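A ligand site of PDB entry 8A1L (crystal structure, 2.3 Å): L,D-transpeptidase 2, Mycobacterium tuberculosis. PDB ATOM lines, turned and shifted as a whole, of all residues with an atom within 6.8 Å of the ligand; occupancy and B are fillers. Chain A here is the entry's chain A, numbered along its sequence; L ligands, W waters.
C11 of the ligand is bonded to SG of Cys 301.
O1 of the ligand lies within hydrogen-bond range of N of Gly 300 (3.4 Å).
The backbone NH of Cys 301 lies within hydrogen-bond range of an oxygen (O1) of the ligand, at 3.0 Å.
The backbone carbonyl oxygen (O) of Gly 279 is in hydrogen-bond range of a nitrogen (N1) of the ligand (2.7 Å).
The backbone NH (N) of Met 250 is in hydrogen-bond range of the backbone carbonyl oxygen (O) of Thr 267 (3.0 Å).
OG of Ser 278 sits at hydrogen-bond distance from OG of Ser 276 (2.6 Å).
OG of Ser 276 sits at hydrogen-bond distance from N of Val 280.
The backbone NH (N) of Phe 281 sits at hydrogen-bond distance from the side-chain sulfur (SG) of Cys 301 (3.4 Å).
The backbone NH (N) of Gly 300 lies within hydrogen-bond range of the side-chain hydroxyl (OG) of Ser 298, at 3.1 Å.
OG of Ser 276 is in hydrogen-bond range of N of Gly 279 (3.1 Å).
The backbone carbonyl oxygen of Tyr 265 lies close to the backbone carbonyl oxygen of Asp 251 (2.5 Å).
The backbone NH (N) of Tyr 265 lies within hydrogen-bond range of the side-chain hydroxyl (OG) of Ser 252 (3.4 Å).
Merely in contact with the ligand: Met 250 (3.7 Å), Asp 251 (3.6 Å), Ser 252 (3.6 Å), Tyr 265 (2.9 Å), Ser 278 (3.9 Å), Val 280 (3.9 Å) and His 299 (3.5 Å).
Hydrophobic or aromatic side chains that line the ligand: Met 250, Val 280 and His 299.
The nearest printed residue that does not touch the ligand is Asn 263 (4.3 Å).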
ATOM      1  N   THR A 232       0.872   3.499  17.191  1.00  0.00           N
ATOM      2  CA  THR A 232       0.884   3.581  15.721  1.00  0.00           C
ATOM      3  C   THR A 232      -0.557   3.512  15.232  1.00  0.00           C
ATOM      4  O   THR A 232      -0.955   2.541  14.568  1.00  0.00           O
ATOM      5  CB  THR A 232       1.728   2.471  15.120  1.00  0.00           C
ATOM      6  OG1 THR A 232       1.269   1.196  15.605  1.00  0.00           O
ATOM      7  CG2 THR A 232       3.191   2.652  15.490  1.00  0.00           C
ATOM      8  N   PRO A 233      -1.351   4.539  15.511  1.00  0.00           N
ATOM      9  CA  PRO A 233      -2.800   4.428  15.274  1.00  0.00           C
ATOM     10  C   PRO A 233      -3.150   4.518  13.797  1.00  0.00           C
ATOM     11  O   PRO A 233      -2.380   5.002  12.965  1.00  0.00           O
ATOM     12  CB  PRO A 233      -3.372   5.614  16.047  1.00  0.00           C
ATOM     13  CG  PRO A 233      -2.280   6.642  15.986  1.00  0.00           C
ATOM     14  CD  PRO A 233      -0.982   5.863  16.035  1.00  0.00           C
ATOM     15  N   MET A 250       4.521  -8.279   3.337  1.00  0.00           N
ATOM     16  CA  MET A 250       4.738  -6.978   3.936  1.00  0.00           C
ATOM     17  C   MET A 250       6.080  -6.992   4.648  1.00  0.00           C
ATOM     18  O   MET A 250       6.292  -7.792   5.577  1.00  0.00           O
ATOM     19  CB  MET A 250       3.602  -6.635   4.908  1.00  0.00           C
ATOM     20  CG  MET A 250       2.215  -6.704   4.260  1.00  0.00           C
ATOM     21  SD  MET A 250       0.881  -6.092   5.298  1.00  0.00           S
ATOM     22  CE  MET A 250      -0.517  -6.282   4.208  1.00  0.00           C
ATOM     23  N   ASP A 251       6.989  -6.118   4.230  1.00  0.00           N
ATOM     24  CA  ASP A 251       8.384  -6.186   4.655  1.00  0.00           C
ATOM     25  C   ASP A 251       8.607  -5.609   6.043  1.00  0.00           C
ATOM     26  O   ASP A 251       8.519  -6.341   7.033  1.00  0.00           O
ATOM     27  CB  ASP A 251       9.280  -5.453   3.639  1.00  0.00           C
ATOM     28  N   SER A 252       8.890  -4.302   6.115  1.00  0.00           N
ATOM     29  CA  SER A 252       9.298  -3.578   7.323  1.00  0.00           C
ATOM     30  C   SER A 252      10.638  -2.906   7.052  1.00  0.00           C
ATOM     31  O   SER A 252      10.789  -1.686   7.239  1.00  0.00           O
ATOM     32  CB  SER A 252       9.423  -4.477   8.559  1.00  0.00           C
ATOM     33  OG  SER A 252       9.865  -3.728   9.682  1.00  0.00           O
ATOM     34  N   SER A 253      11.620  -3.693   6.622  1.00  0.00           N
ATOM     35  CA  SER A 253      12.907  -3.135   6.196  1.00  0.00           C
ATOM     36  C   SER A 253      12.748  -2.191   5.015  1.00  0.00           C
ATOM     37  O   SER A 253      13.629  -1.354   4.780  1.00  0.00           O
ATOM     38  CB  SER A 253      13.877  -4.267   5.854  1.00  0.00           C
ATOM     39  OG  SER A 253      13.202  -5.368   5.277  1.00  0.00           O
ATOM     40  N   THR A 254      11.646  -2.293   4.272  1.00  0.00           N
ATOM     41  CA  THR A 254      11.388  -1.347   3.193  1.00  0.00           C
ATOM     42  C   THR A 254      11.170   0.059   3.716  1.00  0.00           C
ATOM     43  O   THR A 254      11.396   1.034   2.997  1.00  0.00           O
ATOM     44  CB  THR A 254      10.171  -1.795   2.376  1.00  0.00           C
ATOM     45  OG1 THR A 254       9.036  -1.905   3.249  1.00  0.00           O
ATOM     46  N   TYR A 255      10.738   0.189   4.972  1.00  0.00           N
ATOM     47  CA  TYR A 255      10.538   1.485   5.607  1.00  0.00           C
ATOM     48  C   TYR A 255      11.798   1.992   6.302  1.00  0.00           C
ATOM     49  O   TYR A 255      11.771   3.084   6.868  1.00  0.00           O
ATOM     50  CB  TYR A 255       9.395   1.400   6.624  1.00  0.00           C
ATOM     51  N   VAL A 257      13.359   0.432   8.861  1.00  0.00           N
ATOM     52  CA  VAL A 257      13.518  -0.202  10.169  1.00  0.00           C
ATOM     53  C   VAL A 257      13.838  -1.675   9.981  1.00  0.00           C
ATOM     54  O   VAL A 257      13.095  -2.379   9.291  1.00  0.00           O
ATOM     55  CB  VAL A 257      12.252  -0.061  11.033  1.00  0.00           C
ATOM     56  N   ASN A 263      10.621  -2.880  16.725  1.00  0.00           N
ATOM     57  CA  ASN A 263       9.466  -2.399  15.982  1.00  0.00           C
ATOM     58  C   ASN A 263       9.443  -2.881  14.527  1.00  0.00           C
ATOM     59  O   ASN A 263       8.772  -2.274  13.693  1.00  0.00           O
ATOM     60  CB  ASN A 263       9.405  -0.872  16.022  1.00  0.00           C
ATOM     61  CG  ASN A 263       9.504  -0.320  17.429  1.00  0.00           C
ATOM     62  OD1 ASN A 263      10.405  -0.667  18.183  1.00  0.00           O
ATOM     63  ND2 ASN A 263       8.557   0.539  17.782  1.00  0.00           N
ATOM     64  N   GLY A 264      10.162  -3.961  14.217  1.00  0.00           N
ATOM     65  CA  GLY A 264      10.187  -4.503  12.884  1.00  0.00           C
ATOM     66  C   GLY A 264       9.697  -5.939  12.852  1.00  0.00           C
ATOM     67  O   GLY A 264       9.815  -6.674  13.838  1.00  0.00           O
ATOM     68  N   TYR A 265       9.130  -6.333  11.718  1.00  0.00           N
ATOM     69  CA  TYR A 265       8.629  -7.695  11.551  1.00  0.00           C
ATOM     70  C   TYR A 265       8.430  -7.975  10.073  1.00  0.00           C
ATOM     71  O   TYR A 265       8.002  -7.105   9.321  1.00  0.00           O
ATOM     72  CB  TYR A 265       7.317  -7.905  12.317  1.00  0.00           C
ATOM     73  N   ARG A 266       8.745  -9.207   9.663  1.00  0.00           N
ATOM     74  CA  ARG A 266       8.535  -9.680   8.302  1.00  0.00           C
ATOM     75  C   ARG A 266       7.446 -10.744   8.326  1.00  0.00           C
ATOM     76  O   ARG A 266       7.451 -11.641   9.188  1.00  0.00           O
ATOM     77  CB  ARG A 266       9.832 -10.248   7.721  1.00  0.00           C
ATOM     78  CG  ARG A 266       9.649 -11.425   6.758  1.00  0.00           C
ATOM     79  CD  ARG A 266      10.992 -12.028   6.327  1.00  0.00           C
ATOM     80  NE  ARG A 266      11.797 -11.113   5.518  1.00  0.00           N
ATOM     81  CZ  ARG A 266      12.944 -10.545   5.908  1.00  0.00           C
ATOM     82  NH1 ARG A 266      13.450 -10.788   7.111  1.00  0.00           N
ATOM     83  NH2 ARG A 266      13.573  -9.727   5.083  1.00  0.00           N
ATOM     84  N   THR A 267       6.512 -10.670   7.378  1.00  0.00           N
ATOM     85  CA  THR A 267       5.406 -11.623   7.369  1.00  0.00           C
ATOM     86  C   THR A 267       4.689 -11.575   6.028  1.00  0.00           C
ATOM     87  O   THR A 267       4.599 -10.524   5.395  1.00  0.00           O
ATOM     88  CB  THR A 267       4.417 -11.323   8.504  1.00  0.00           C
ATOM     89  OG1 THR A 267       3.209 -12.063   8.303  1.00  0.00           O
ATOM     90  CG2 THR A 267       4.084  -9.840   8.551  1.00  0.00           C
ATOM     91  N   VAL A 269       1.051 -12.209   4.176  1.00  0.00           N
ATOM     92  CA  VAL A 269      -0.313 -11.968   4.640  1.00  0.00           C
ATOM     93  C   VAL A 269      -1.304 -12.447   3.588  1.00  0.00           C
ATOM     94  O   VAL A 269      -1.096 -12.241   2.395  1.00  0.00           O
ATOM     95  CB  VAL A 269      -0.531 -10.473   4.941  1.00  0.00           C
ATOM     96  CG1 VAL A 269      -1.992 -10.187   5.213  1.00  0.00           C
ATOM     97  CG2 VAL A 269       0.335 -10.042   6.113  1.00  0.00           C
ATOM     98  N   SER A 276      -4.475   2.234   1.207  1.00  0.00           N
ATOM     99  CA  SER A 276      -3.646   3.427   1.266  1.00  0.00           C
ATOM    100  C   SER A 276      -2.268   3.109   0.714  1.00  0.00           C
ATOM    101  O   SER A 276      -1.752   1.993   0.902  1.00  0.00           O
ATOM    102  CB  SER A 276      -3.523   3.955   2.705  1.00  0.00           C
ATOM    103  OG  SER A 276      -2.441   3.362   3.403  1.00  0.00           O
ATOM    104  N   TYR A 277      -1.667   4.087   0.029  1.00  0.00           N
ATOM    105  CA  TYR A 277      -0.287   3.938  -0.402  1.00  0.00           C
ATOM    106  C   TYR A 277       0.644   3.780   0.798  1.00  0.00           C
ATOM    107  O   TYR A 277       1.726   3.199   0.673  1.00  0.00           O
ATOM    108  CB  TYR A 277       0.158   5.151  -1.235  1.00  0.00           C
ATOM    109  CG  TYR A 277      -0.322   5.186  -2.677  1.00  0.00           C
ATOM    110  CD1 TYR A 277      -1.486   4.533  -3.057  1.00  0.00           C
ATOM    111  CD2 TYR A 277       0.394   5.869  -3.651  1.00  0.00           C
ATOM    112  CE1 TYR A 277      -1.926   4.562  -4.370  1.00  0.00           C
ATOM    113  CE2 TYR A 277      -0.037   5.909  -4.965  1.00  0.00           C
ATOM    114  CZ  TYR A 277      -1.197   5.238  -5.317  1.00  0.00           C
ATOM    115  OH  TYR A 277      -1.631   5.273  -6.623  1.00  0.00           O
ATOM    116  N   SER A 278       0.247   4.317   1.954  1.00  0.00           N
ATOM    117  CA  SER A 278       1.084   4.270   3.139  1.00  0.00           C
ATOM    118  C   SER A 278       1.177   2.865   3.745  1.00  0.00           C
ATOM    119  O   SER A 278       2.000   2.653   4.626  1.00  0.00           O
ATOM    120  CB  SER A 278       0.562   5.242   4.199  1.00  0.00           C
ATOM    121  OG  SER A 278      -0.779   4.947   4.554  1.00  0.00           O
ATOM    122  N   GLY A 279       0.353   1.926   3.284  1.00  0.00           N
ATOM    123  CA  GLY A 279       0.457   0.542   3.688  1.00  0.00           C
ATOM    124  C   GLY A 279      -0.705  -0.002   4.502  1.00  0.00           C
ATOM    125  O   GLY A 279      -0.567  -1.092   5.064  1.00  0.00           O
ATOM    126  N   VAL A 280      -1.814   0.713   4.581  1.00  0.00           N
ATOM    127  CA  VAL A 280      -2.967   0.238   5.344  1.00  0.00           C
ATOM    128  C   VAL A 280      -3.732  -0.780   4.501  1.00  0.00           C
ATOM    129  O   VAL A 280      -4.152  -0.478   3.378  1.00  0.00           O
ATOM    130  CB  VAL A 280      -3.864   1.395   5.774  1.00  0.00           C
ATOM    131  CG1 VAL A 280      -5.118   0.874   6.474  1.00  0.00           C
ATOM    132  CG2 VAL A 280      -3.102   2.333   6.689  1.00  0.00           C
ATOM    133  N   PHE A 281      -3.931  -1.974   5.052  1.00  0.00           N
ATOM    134  CA  PHE A 281      -4.631  -3.057   4.386  1.00  0.00           C
ATOM    135  C   PHE A 281      -5.754  -3.580   5.259  1.00  0.00           C
ATOM    136  O   PHE A 281      -5.703  -3.496   6.496  1.00  0.00           O
ATOM    137  CB  PHE A 281      -3.681  -4.234   4.069  1.00  0.00           C
ATOM    138  CG  PHE A 281      -2.744  -3.980   2.926  1.00  0.00           C
ATOM    139  CD1 PHE A 281      -1.596  -3.230   3.108  1.00  0.00           C
ATOM    140  CD2 PHE A 281      -2.988  -4.531   1.677  1.00  0.00           C
ATOM    141  CE1 PHE A 281      -0.719  -3.017   2.053  1.00  0.00           C
ATOM    142  CE2 PHE A 281      -2.118  -4.312   0.624  1.00  0.00           C
ATOM    143  CZ  PHE A 281      -0.989  -3.555   0.816  1.00  0.00           C
ATOM    144  N   HIS A 283      -6.897  -7.148   5.930  1.00  0.00           N
ATOM    145  CA  HIS A 283      -6.211  -8.404   5.677  1.00  0.00           C
ATOM    146  C   HIS A 283      -6.521  -9.420   6.760  1.00  0.00           C
ATOM    147  O   HIS A 283      -7.032  -9.102   7.841  1.00  0.00           O
ATOM    148  CB  HIS A 283      -4.701  -8.192   5.596  1.00  0.00           C
ATOM    149  CG  HIS A 283      -4.078  -7.794   6.899  1.00  0.00           C
ATOM    150  ND1 HIS A 283      -3.506  -8.701   7.765  1.00  0.00           N
ATOM    151  CD2 HIS A 283      -3.963  -6.584   7.493  1.00  0.00           C
ATOM    152  CE1 HIS A 283      -3.054  -8.069   8.823  1.00  0.00           C
ATOM    153  NE2 HIS A 283      -3.314  -6.780   8.687  1.00  0.00           N
ATOM    154  N   SER A 298      -2.582  -3.513  15.962  1.00  0.00           N
ATOM    155  CA  SER A 298      -1.828  -3.508  14.719  1.00  0.00           C
ATOM    156  C   SER A 298      -0.890  -2.302  14.653  1.00  0.00           C
ATOM    157  O   SER A 298      -0.760  -1.533  15.604  1.00  0.00           O
ATOM    158  CB  SER A 298      -2.771  -3.523  13.522  1.00  0.00           C
ATOM    159  OG  SER A 298      -3.319  -2.232  13.289  1.00  0.00           O
ATOM    160  N   HIS A 299      -0.230  -2.144  13.504  1.00  0.00           N
ATOM    161  CA  HIS A 299       0.597  -0.985  13.227  1.00  0.00           C
ATOM    162  C   HIS A 299      -0.131   0.061  12.379  1.00  0.00           C
ATOM    163  O   HIS A 299       0.469   1.085  12.037  1.00  0.00           O
ATOM    164  CB  HIS A 299       1.877  -1.421  12.498  1.00  0.00           C
ATOM    165  CG  HIS A 299       2.858  -2.136  13.377  1.00  0.00           C
ATOM    166  ND1 HIS A 299       4.082  -1.604  13.698  1.00  0.00           N
ATOM    167  CD2 HIS A 299       2.787  -3.344  13.986  1.00  0.00           C
ATOM    168  CE1 HIS A 299       4.736  -2.443  14.478  1.00  0.00           C
ATOM    169  NE2 HIS A 299       3.964  -3.503  14.668  1.00  0.00           N
ATOM    170  N   GLY A 300      -1.391  -0.180  12.041  1.00  0.00           N
ATOM    171  CA  GLY A 300      -2.143   0.728  11.189  1.00  0.00           C
ATOM    172  C   GLY A 300      -3.142  -0.036  10.347  1.00  0.00           C
ATOM    173  O   GLY A 300      -4.201   0.473   9.989  1.00  0.00           O
ATOM    174  N   CYS A 301      -2.802  -1.286  10.026  1.00  0.00           N
ATOM    175  CA  CYS A 301      -3.646  -2.095   9.245  1.00  0.00           C
ATOM    176  C   CYS A 301      -4.953  -2.450   9.975  1.00  0.00           C
ATOM    177  O   CYS A 301      -4.995  -2.429  11.205  1.00  0.00           O
ATOM    178  CB  CYS A 301      -2.914  -3.441   8.934  1.00  0.00           C
ATOM    179  SG  CYS A 301      -1.850  -3.271   7.450  1.00  0.00           S
ATOM    180  N   LEU A 302      -5.982  -2.777   9.221  1.00  0.00           N
ATOM    181  CA  LEU A 302      -7.263  -3.241   9.768  1.00  0.00           C
ATOM    182  C   LEU A 302      -7.257  -4.762   9.851  1.00  0.00           C
ATOM    183  O   LEU A 302      -7.578  -5.443   8.880  1.00  0.00           O
ATOM    184  CB  LEU A 302      -8.429  -2.737   8.919  1.00  0.00           C
ATOM    185  CG  LEU A 302      -8.878  -1.307   9.177  1.00  0.00           C
ATOM    186  CD1 LEU A 302      -7.725  -0.330   9.107  1.00  0.00           C
ATOM    187  CD2 LEU A 302      -9.969  -0.909   8.195  1.00  0.00           C
ATOM    188  N   ASN A 303      -6.862  -5.276  11.022  1.00  0.00           N
ATOM    189  CA  ASN A 303      -6.851  -6.721  11.226  1.00  0.00           C
ATOM    190  C   ASN A 303      -8.271  -7.251  11.315  1.00  0.00           C
ATOM    191  O   ASN A 303      -9.110  -6.691  12.024  1.00  0.00           O
ATOM    192  CB  ASN A 303      -6.083  -7.057  12.502  1.00  0.00           C
ATOM    193  CG  ASN A 303      -4.587  -6.869  12.359  1.00  0.00           C
ATOM    194  OD1 ASN A 303      -4.114  -6.303  11.367  1.00  0.00           O
ATOM    195  ND2 ASN A 303      -3.829  -7.336  13.344  1.00  0.00           N
HETATM  196  C1  LIG L   1       2.701  -2.301   5.700  1.00  0.00           C
HETATM  197  C2  LIG L   1       4.879  -2.415   6.689  1.00  0.00           C
HETATM  198  C3  LIG L   1       5.945  -5.121   9.237  1.00  0.00           C
HETATM  199  C4  LIG L   1       6.336  -4.334  10.339  1.00  0.00           C
HETATM  200  C5  LIG L   1       6.271  -2.930  10.252  1.00  0.00           C
HETATM  201  C6  LIG L   1       0.447   1.987   8.315  1.00  0.00           C
HETATM  202  C7  LIG L   1       0.665   0.613   7.620  1.00  0.00           C
HETATM  203  C8  LIG L   1       1.746  -0.222   8.341  1.00  0.00           C
HETATM  204  C9  LIG L   1       1.698  -1.689   7.946  1.00  0.00           C
HETATM  205  C10 LIG L   1       0.498  -2.388   8.595  1.00  0.00           C
HETATM  206  C11 LIG L   1      -0.130  -3.633   7.911  1.00  0.00           C
HETATM  207  C12 LIG L   1       5.418  -3.100   8.010  1.00  0.00           C
HETATM  208  C13 LIG L   1       5.485  -4.516   8.090  1.00  0.00           C
HETATM  209  C14 LIG L   1       5.801  -2.318   9.092  1.00  0.00           C
HETATM  210  C15 LIG L   1       3.188   0.414   8.076  1.00  0.00           C
HETATM  211  N1  LIG L   1       1.580  -1.800   6.504  1.00  0.00           N
HETATM  212  O1  LIG L   1       0.055  -2.007   9.608  1.00  0.00           O
HETATM  213  O2  LIG L   1       3.711  -3.104   6.296  1.00  0.00           O
HETATM  214  O3  LIG L   1       2.773  -2.045   4.535  1.00  0.00           O
HETATM  215  O   HOH W   1       5.302   3.136   7.992  1.00  0.00           O
HETATM  216  O   HOH W   2       3.340  -3.219  10.534  1.00  0.00           O
